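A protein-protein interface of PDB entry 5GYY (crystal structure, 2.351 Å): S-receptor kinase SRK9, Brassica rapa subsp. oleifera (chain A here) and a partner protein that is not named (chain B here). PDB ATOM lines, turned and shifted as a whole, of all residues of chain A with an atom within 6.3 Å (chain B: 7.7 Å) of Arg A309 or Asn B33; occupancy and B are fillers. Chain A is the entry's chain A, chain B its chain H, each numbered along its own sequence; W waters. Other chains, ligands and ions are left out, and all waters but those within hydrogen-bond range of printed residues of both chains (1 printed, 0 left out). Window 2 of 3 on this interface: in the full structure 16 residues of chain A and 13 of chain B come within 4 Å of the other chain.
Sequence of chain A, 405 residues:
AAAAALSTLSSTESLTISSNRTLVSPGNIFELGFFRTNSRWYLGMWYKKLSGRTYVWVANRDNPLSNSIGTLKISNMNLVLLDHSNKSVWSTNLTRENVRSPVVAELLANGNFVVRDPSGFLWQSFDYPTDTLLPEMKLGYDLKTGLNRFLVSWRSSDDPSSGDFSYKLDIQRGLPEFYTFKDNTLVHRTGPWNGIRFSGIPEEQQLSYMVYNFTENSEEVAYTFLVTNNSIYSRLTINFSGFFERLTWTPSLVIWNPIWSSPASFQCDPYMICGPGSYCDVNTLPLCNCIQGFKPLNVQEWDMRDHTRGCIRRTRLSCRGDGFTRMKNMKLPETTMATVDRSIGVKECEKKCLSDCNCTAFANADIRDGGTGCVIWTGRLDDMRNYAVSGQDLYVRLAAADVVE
Of the 13 printed residues of chain B, 4 touch a printed residue of chain A.
Among the printed residues, 8 pairs touch across the chains.
OD1 of Asn A298 lies within hydrogen-bond range of N of Glu A301 (3.2 Å).
The backbone carbonyl oxygen of Glu A301 is in hydrogen-bond range of the backbone NH of Asp A306, at 2.8 Å.
The side-chain carboxylate (OE2) of Glu A301 is in salt-bridge range of the guanidinium group (NH1) of Arg A309 (2.8 Å).
The side-chain hydroxyl (OG1) of Thr A308 is in hydrogen-bond range of the side-chain carboxylate (OD1) of Asp A306.
The side-chain amide oxygen of Asn B33 lies within hydrogen-bond range of the side-chain amino group of Lys B34 (2.7 Å).
Arg A309 touches two residues of chain B.
Of chain A, only Glu A301 and Arg A309 come within 4 Å of Asn B33.
No residue of chain B comes within 4 Å of Gly A310.
Printed residues of chain A within 4 Å of Phe B30: Thr A308 (3.2 Å).
Printed residues of chain A within 4 Å of Leu B13: Thr A308 (3.6 Å).
Printed residues of chain B within 4 Å of Thr A308: Leu B13 (3.6 Å), Phe B30 (3.2 Å) and Lys B34 (3.5 Å).
Of the printed residues of chain B, Glu A301 touches Asn B33 (3.6 Å) and Lys B34 (2.6 Å).
Pro A276 touches none of the printed residues of chain B.
The nearest residue of chain B that does not touch Arg A309 is Thr B35 (4.9 Å).
The side-chain carboxylate (OE2) of Glu A301 lies within salt-bridge range of the side-chain amino group (NZ) of Lys B34 (2.6 Å).
OD2 of Asp A306 lies within salt-bridge range of NZ of Lys B34, 2.7 Å away.
The guanidinium group (NH2) of Arg A309 is in hydrogen-bond range of the backbone carbonyl oxygen (O) of Lys B34.
Water W1 lies within hydrogen-bond range of the guanidinium group of Arg A309 (2.7 Å), the backbone carbonyl oxygen of Asn B33 (2.8 Å), the backbone carbonyl oxygen of Lys B34 (3.1 Å) and the side-chain amide nitrogen of Asn B36 (3.2 Å).
Glu A301 touches Asn B33.
CD2 of Leu B13 touches CG2 of Thr A308, 3.6 Å away.
Thr A308 touches Phe B30 (OG1 to CZ, 3.2 Å).
CE of Lys B34 touches CB of Thr A308 (3.5 Å).
NH2 of Arg A309 touches O of Asn B33 (3.8 Å).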
ATOM      1  N   GLY A 275     -10.188  19.848  22.693  1.00  0.00           N
ATOM      2  CA  GLY A 275     -11.565  20.273  22.881  1.00  0.00           C
ATOM      3  C   GLY A 275     -12.471  19.212  23.506  1.00  0.00           C
ATOM      4  O   GLY A 275     -12.029  18.100  23.815  1.00  0.00           O
ATOM      5  N   PRO A 276     -13.759  19.545  23.675  1.00  0.00           N
ATOM      6  CA  PRO A 276     -14.776  18.651  24.250  1.00  0.00           C
ATOM      7  C   PRO A 276     -14.931  17.332  23.481  1.00  0.00           C
ATOM      8  O   PRO A 276     -14.882  17.315  22.242  1.00  0.00           O
ATOM      9  CB  PRO A 276     -16.067  19.469  24.136  1.00  0.00           C
ATOM     10  CG  PRO A 276     -15.621  20.873  23.977  1.00  0.00           C
ATOM     11  CD  PRO A 276     -14.331  20.831  23.250  1.00  0.00           C
ATOM     12  N   LEU A 297     -15.840  17.823  15.178  1.00  0.00           N
ATOM     13  CA  LEU A 297     -16.874  18.784  14.829  1.00  0.00           C
ATOM     14  C   LEU A 297     -16.526  19.558  13.552  1.00  0.00           C
ATOM     15  O   LEU A 297     -17.407  19.951  12.789  1.00  0.00           O
ATOM     16  CB  LEU A 297     -17.070  19.755  15.990  1.00  0.00           C
ATOM     17  CG  LEU A 297     -18.396  20.501  16.173  1.00  0.00           C
ATOM     18  CD1 LEU A 297     -18.542  20.861  17.632  1.00  0.00           C
ATOM     19  CD2 LEU A 297     -18.482  21.753  15.320  1.00  0.00           C
ATOM     20  N   ASN A 298     -15.236  19.769  13.322  1.00  0.00           N
ATOM     21  CA  ASN A 298     -14.767  20.509  12.156  1.00  0.00           C
ATOM     22  C   ASN A 298     -13.543  19.820  11.561  1.00  0.00           C
ATOM     23  O   ASN A 298     -12.440  19.942  12.087  1.00  0.00           O
ATOM     24  CB  ASN A 298     -14.467  21.964  12.550  1.00  0.00           C
ATOM     25  CG  ASN A 298     -14.149  22.861  11.352  1.00  0.00           C
ATOM     26  OD1 ASN A 298     -13.590  22.417  10.354  1.00  0.00           O
ATOM     27  ND2 ASN A 298     -14.502  24.140  11.463  1.00  0.00           N
ATOM     28  N   GLU A 301     -10.449  22.033  10.325  1.00  0.00           N
ATOM     29  CA  GLU A 301      -9.665  22.460  11.473  1.00  0.00           C
ATOM     30  C   GLU A 301      -8.940  21.283  12.102  1.00  0.00           C
ATOM     31  O   GLU A 301      -7.764  21.389  12.455  1.00  0.00           O
ATOM     32  CB  GLU A 301     -10.537  23.184  12.499  1.00  0.00           C
ATOM     33  CG  GLU A 301     -10.915  24.579  12.058  1.00  0.00           C
ATOM     34  CD  GLU A 301     -11.827  25.282  13.040  1.00  0.00           C
ATOM     35  OE1 GLU A 301     -12.327  24.612  13.970  1.00  0.00           O
ATOM     36  OE2 GLU A 301     -12.035  26.508  12.888  1.00  0.00           O
ATOM     37  N   TRP A 302      -9.628  20.154  12.217  1.00  0.00           N
ATOM     38  CA  TRP A 302      -9.026  18.983  12.841  1.00  0.00           C
ATOM     39  C   TRP A 302      -7.790  18.471  12.087  1.00  0.00           C
ATOM     40  O   TRP A 302      -6.806  18.069  12.703  1.00  0.00           O
ATOM     41  CB  TRP A 302     -10.043  17.857  12.990  1.00  0.00           C
ATOM     42  CG  TRP A 302      -9.653  16.908  14.081  1.00  0.00           C
ATOM     43  CD1 TRP A 302      -8.939  15.761  13.947  1.00  0.00           C
ATOM     44  CD2 TRP A 302      -9.950  17.039  15.479  1.00  0.00           C
ATOM     45  NE1 TRP A 302      -8.766  15.164  15.177  1.00  0.00           N
ATOM     46  CE2 TRP A 302      -9.381  15.931  16.132  1.00  0.00           C
ATOM     47  CE3 TRP A 302     -10.645  17.986  16.239  1.00  0.00           C
ATOM     48  CZ2 TRP A 302      -9.495  15.734  17.509  1.00  0.00           C
ATOM     49  CZ3 TRP A 302     -10.744  17.800  17.609  1.00  0.00           C
ATOM     50  CH2 TRP A 302     -10.167  16.682  18.229  1.00  0.00           C
ATOM     51  N   ASP A 306      -6.021  21.903  14.613  1.00  0.00           N
ATOM     52  CA  ASP A 306      -6.820  22.844  15.389  1.00  0.00           C
ATOM     53  C   ASP A 306      -7.885  22.009  16.081  1.00  0.00           C
ATOM     54  O   ASP A 306      -8.895  21.676  15.469  1.00  0.00           O
ATOM     55  CB  ASP A 306      -7.499  23.853  14.460  1.00  0.00           C
ATOM     56  CG  ASP A 306      -8.395  24.846  15.202  1.00  0.00           C
ATOM     57  OD1 ASP A 306      -8.709  24.627  16.394  1.00  0.00           O
ATOM     58  OD2 ASP A 306      -8.812  25.847  14.572  1.00  0.00           O
ATOM     59  N   HIS A 307      -7.673  21.684  17.354  1.00  0.00           N
ATOM     60  CA  HIS A 307      -8.579  20.771  18.058  1.00  0.00           C
ATOM     61  C   HIS A 307      -9.590  21.478  18.965  1.00  0.00           C
ATOM     62  O   HIS A 307     -10.301  20.825  19.740  1.00  0.00           O
ATOM     63  CB  HIS A 307      -7.773  19.741  18.849  1.00  0.00           C
ATOM     64  CG  HIS A 307      -6.843  18.938  17.998  1.00  0.00           C
ATOM     65  ND1 HIS A 307      -7.295  18.026  17.070  1.00  0.00           N
ATOM     66  CD2 HIS A 307      -5.492  18.938  17.905  1.00  0.00           C
ATOM     67  CE1 HIS A 307      -6.259  17.488  16.451  1.00  0.00           C
ATOM     68  NE2 HIS A 307      -5.153  18.019  16.942  1.00  0.00           N
ATOM     69  N   THR A 308      -9.664  22.801  18.824  1.00  0.00           N
ATOM     70  CA  THR A 308     -10.447  23.677  19.701  1.00  0.00           C
ATOM     71  C   THR A 308     -11.901  23.237  19.858  1.00  0.00           C
ATOM     72  O   THR A 308     -12.389  23.093  20.982  1.00  0.00           O
ATOM     73  CB  THR A 308     -10.460  25.136  19.165  1.00  0.00           C
ATOM     74  OG1 THR A 308      -9.163  25.496  18.670  1.00  0.00           O
ATOM     75  CG2 THR A 308     -10.892  26.108  20.247  1.00  0.00           C
ATOM     76  N   ARG A 309     -12.577  22.998  18.737  1.00  0.00           N
ATOM     77  CA  ARG A 309     -13.999  22.652  18.761  1.00  0.00           C
ATOM     78  C   ARG A 309     -14.285  21.250  19.317  1.00  0.00           C
ATOM     79  O   ARG A 309     -15.394  20.969  19.770  1.00  0.00           O
ATOM     80  CB  ARG A 309     -14.603  22.780  17.360  1.00  0.00           C
ATOM     81  CG  ARG A 309     -14.372  24.118  16.723  1.00  0.00           C
ATOM     82  CD  ARG A 309     -14.993  24.168  15.353  1.00  0.00           C
ATOM     83  NE  ARG A 309     -15.919  25.284  15.268  1.00  0.00           N
ATOM     84  CZ  ARG A 309     -15.679  26.438  14.666  1.00  0.00           C
ATOM     85  NH1 ARG A 309     -14.523  26.663  14.057  1.00  0.00           N
ATOM     86  NH2 ARG A 309     -16.621  27.366  14.667  1.00  0.00           N
ATOM     87  N   GLY A 310     -13.287  20.374  19.273  1.00  0.00           N
ATOM     88  CA  GLY A 310     -13.445  19.030  19.795  1.00  0.00           C
ATOM     89  C   GLY A 310     -14.286  18.108  18.927  1.00  0.00           C
ATOM     90  O   GLY A 310     -14.432  18.316  17.723  1.00  0.00           O
ATOM     91  N   CYS A 311     -14.866  17.094  19.558  1.00  0.00           N
ATOM     92  CA  CYS A 311     -15.585  16.065  18.833  1.00  0.00           C
ATOM     93  C   CYS A 311     -17.017  15.917  19.333  1.00  0.00           C
ATOM     94  O   CYS A 311     -17.342  16.366  20.425  1.00  0.00           O
ATOM     95  CB  CYS A 311     -14.838  14.730  18.960  1.00  0.00           C
ATOM     96  SG  CYS A 311     -13.114  14.819  18.398  1.00  0.00           S
ATOM     97  N   ILE A 312     -17.871  15.315  18.509  1.00  0.00           N
ATOM     98  CA  ILE A 312     -19.249  14.989  18.893  1.00  0.00           C
ATOM     99  C   ILE A 312     -19.578  13.552  18.503  1.00  0.00           C
ATOM    100  O   ILE A 312     -18.881  12.943  17.691  1.00  0.00           O
ATOM    101  CB  ILE A 312     -20.298  15.913  18.244  1.00  0.00           C
ATOM    102  CG1 ILE A 312     -20.196  15.861  16.718  1.00  0.00           C
ATOM    103  CG2 ILE A 312     -20.147  17.340  18.754  1.00  0.00           C
ATOM    104  CD1 ILE A 312     -21.341  16.573  16.011  1.00  0.00           C
ATOM    105  N   LEU B  13     -10.305  29.920  25.390  1.00  0.00           N
ATOM    106  CA  LEU B  13      -9.767  29.233  24.205  1.00  0.00           C
ATOM    107  C   LEU B  13      -8.246  29.053  24.266  1.00  0.00           C
ATOM    108  O   LEU B  13      -7.498  30.035  24.226  1.00  0.00           O
ATOM    109  CB  LEU B  13     -10.131  29.978  22.923  1.00  0.00           C
ATOM    110  CG  LEU B  13     -11.617  30.113  22.612  1.00  0.00           C
ATOM    111  CD1 LEU B  13     -11.835  31.021  21.415  1.00  0.00           C
ATOM    112  CD2 LEU B  13     -12.238  28.741  22.377  1.00  0.00           C
ATOM    113  N   ASP B  26      -4.699  38.637  18.451  1.00  0.00           N
ATOM    114  CA  ASP B  26      -4.756  37.292  17.892  1.00  0.00           C
ATOM    115  C   ASP B  26      -5.880  36.487  18.519  1.00  0.00           C
ATOM    116  O   ASP B  26      -6.644  35.834  17.816  1.00  0.00           O
ATOM    117  CB  ASP B  26      -3.422  36.562  18.083  1.00  0.00           C
ATOM    118  CG  ASP B  26      -2.296  37.185  17.271  1.00  0.00           C
ATOM    119  OD1 ASP B  26      -2.606  37.901  16.291  1.00  0.00           O
ATOM    120  OD2 ASP B  26      -1.112  36.940  17.605  1.00  0.00           O
ATOM    121  N   CYS B  27      -5.951  36.537  19.845  1.00  0.00           N
ATOM    122  CA  CYS B  27      -7.013  35.914  20.614  1.00  0.00           C
ATOM    123  C   CYS B  27      -8.393  36.401  20.188  1.00  0.00           C
ATOM    124  O   CYS B  27      -9.328  35.609  20.084  1.00  0.00           O
ATOM    125  CB  CYS B  27      -6.824  36.185  22.109  1.00  0.00           C
ATOM    126  SG  CYS B  27      -5.600  35.168  22.953  1.00  0.00           S
ATOM    127  N   GLU B  28      -8.529  37.706  19.965  1.00  0.00           N
ATOM    128  CA  GLU B  28      -9.828  38.283  19.611  1.00  0.00           C
ATOM    129  C   GLU B  28     -10.302  37.776  18.249  1.00  0.00           C
ATOM    130  O   GLU B  28     -11.499  37.569  18.031  1.00  0.00           O
ATOM    131  CB  GLU B  28      -9.788  39.813  19.668  1.00  0.00           C
ATOM    132  CG  GLU B  28      -9.734  40.356  21.103  1.00  0.00           C
ATOM    133  CD  GLU B  28      -9.261  41.803  21.203  1.00  0.00           C
ATOM    134  OE1 GLU B  28      -9.191  42.491  20.160  1.00  0.00           O
ATOM    135  OE2 GLU B  28      -8.961  42.251  22.334  1.00  0.00           O
ATOM    136  N   ALA B  29      -9.351  37.586  17.340  1.00  0.00           N
ATOM    137  CA  ALA B  29      -9.618  37.025  16.021  1.00  0.00           C
ATOM    138  C   ALA B  29      -9.966  35.554  16.130  1.00  0.00           C
ATOM    139  O   ALA B  29     -10.875  35.070  15.457  1.00  0.00           O
ATOM    140  CB  ALA B  29      -8.392  37.221  15.091  1.00  0.00           C
ATOM    141  N   PHE B  30      -9.226  34.853  16.985  1.00  0.00           N
ATOM    142  CA  PHE B  30      -9.446  33.435  17.242  1.00  0.00           C
ATOM    143  C   PHE B  30     -10.882  33.226  17.759  1.00  0.00           C
ATOM    144  O   PHE B  30     -11.579  32.303  17.340  1.00  0.00           O
ATOM    145  CB  PHE B  30      -8.401  32.922  18.252  1.00  0.00           C
ATOM    146  CG  PHE B  30      -8.399  31.416  18.438  1.00  0.00           C
ATOM    147  CD1 PHE B  30      -8.921  30.573  17.471  1.00  0.00           C
ATOM    148  CD2 PHE B  30      -7.867  30.849  19.594  1.00  0.00           C
ATOM    149  CE1 PHE B  30      -8.916  29.179  17.647  1.00  0.00           C
ATOM    150  CE2 PHE B  30      -7.857  29.467  19.783  1.00  0.00           C
ATOM    151  CZ  PHE B  30      -8.383  28.630  18.807  1.00  0.00           C
ATOM    152  N   TYR B  31     -11.316  34.097  18.666  1.00  0.00           N
ATOM    153  CA  TYR B  31     -12.665  34.048  19.214  1.00  0.00           C
ATOM    154  C   TYR B  31     -13.710  34.199  18.110  1.00  0.00           C
ATOM    155  O   TYR B  31     -14.643  33.419  18.025  1.00  0.00           O
ATOM    156  CB  TYR B  31     -12.864  35.137  20.287  1.00  0.00           C
ATOM    157  CG  TYR B  31     -14.284  35.209  20.817  1.00  0.00           C
ATOM    158  CD1 TYR B  31     -14.728  34.333  21.806  1.00  0.00           C
ATOM    159  CD2 TYR B  31     -15.190  36.133  20.305  1.00  0.00           C
ATOM    160  CE1 TYR B  31     -16.029  34.385  22.277  1.00  0.00           C
ATOM    161  CE2 TYR B  31     -16.493  36.194  20.772  1.00  0.00           C
ATOM    162  CZ  TYR B  31     -16.906  35.320  21.759  1.00  0.00           C
ATOM    163  OH  TYR B  31     -18.199  35.387  22.223  1.00  0.00           O
ATOM    164  N   THR B  32     -13.553  35.233  17.289  1.00  0.00           N
ATOM    165  CA  THR B  32     -14.470  35.519  16.194  1.00  0.00           C
ATOM    166  C   THR B  32     -14.573  34.341  15.237  1.00  0.00           C
ATOM    167  O   THR B  32     -15.674  33.948  14.859  1.00  0.00           O
ATOM    168  CB  THR B  32     -14.042  36.800  15.424  1.00  0.00           C
ATOM    169  OG1 THR B  32     -13.978  37.909  16.333  1.00  0.00           O
ATOM    170  CG2 THR B  32     -15.030  37.126  14.318  1.00  0.00           C
ATOM    171  N   ASN B  33     -13.428  33.782  14.850  1.00  0.00           N
ATOM    172  CA  ASN B  33     -13.402  32.610  13.974  1.00  0.00           C
ATOM    173  C   ASN B  33     -14.137  31.412  14.584  1.00  0.00           C
ATOM    174  O   ASN B  33     -14.792  30.630  13.878  1.00  0.00           O
ATOM    175  CB  ASN B  33     -11.958  32.227  13.623  1.00  0.00           C
ATOM    176  CG  ASN B  33     -11.805  30.753  13.251  1.00  0.00           C
ATOM    177  OD1 ASN B  33     -11.538  29.905  14.107  1.00  0.00           O
ATOM    178  ND2 ASN B  33     -11.955  30.448  11.962  1.00  0.00           N
ATOM    179  N   LYS B  34     -14.026  31.272  15.900  1.00  0.00           N
ATOM    180  CA  LYS B  34     -14.624  30.139  16.591  1.00  0.00           C
ATOM    181  C   LYS B  34     -16.106  30.325  16.971  1.00  0.00           C
ATOM    182  O   LYS B  34     -16.821  29.344  17.133  1.00  0.00           O
ATOM    183  CB  LYS B  34     -13.775  29.758  17.809  1.00  0.00           C
ATOM    184  CG  LYS B  34     -12.462  29.066  17.455  1.00  0.00           C
ATOM    185  CD  LYS B  34     -12.709  27.736  16.748  1.00  0.00           C
ATOM    186  CE  LYS B  34     -11.406  27.028  16.348  1.00  0.00           C
ATOM    187  NZ  LYS B  34     -10.924  27.492  15.020  1.00  0.00           N
ATOM    188  N   THR B  35     -16.564  31.569  17.101  1.00  0.00           N
ATOM    189  CA  THR B  35     -17.935  31.844  17.564  1.00  0.00           C
ATOM    190  C   THR B  35     -18.824  32.672  16.632  1.00  0.00           C
ATOM    191  O   THR B  35     -20.037  32.718  16.826  1.00  0.00           O
ATOM    192  CB  THR B  35     -17.957  32.590  18.915  1.00  0.00           C
ATOM    193  OG1 THR B  35     -17.264  33.839  18.774  1.00  0.00           O
ATOM    194  CG2 THR B  35     -17.313  31.782  20.021  1.00  0.00           C
ATOM    195  N   ASN B  36     -18.228  33.326  15.641  1.00  0.00           N
ATOM    196  CA  ASN B  36     -18.954  34.243  14.760  1.00  0.00           C
ATOM    197  C   ASN B  36     -19.488  35.460  15.505  1.00  0.00           C
ATOM    198  O   ASN B  36     -20.343  36.185  15.005  1.00  0.00           O
ATOM    199  CB  ASN B  36     -20.067  33.547  13.983  1.00  0.00           C
ATOM    200  CG  ASN B  36     -19.596  33.042  12.647  1.00  0.00           C
ATOM    201  OD1 ASN B  36     -19.324  33.829  11.742  1.00  0.00           O
ATOM    202  ND2 ASN B  36     -19.474  31.724  12.514  1.00  0.00           N
ATOM    203  N   GLN B  37     -18.960  35.674  16.702  1.00  0.00           N
ATOM    204  CA  GLN B  37     -19.280  36.846  17.486  1.00  0.00           C
ATOM    205  C   GLN B  37     -18.007  37.616  17.758  1.00  0.00           C
ATOM    206  O   GLN B  37     -16.917  37.146  17.438  1.00  0.00           O
ATOM    207  CB  GLN B  37     -19.926  36.456  18.812  1.00  0.00           C
ATOM    208  CG  GLN B  37     -21.113  35.519  18.705  1.00  0.00           C
ATOM    209  CD  GLN B  37     -21.767  35.310  20.056  1.00  0.00           C
ATOM    210  OE1 GLN B  37     -21.846  36.233  20.862  1.00  0.00           O
ATOM    211  NE2 GLN B  37     -22.222  34.091  20.317  1.00  0.00           N
HETATM  212  O   HOH W   1     -17.485  29.809  14.094  1.00  0.00           O
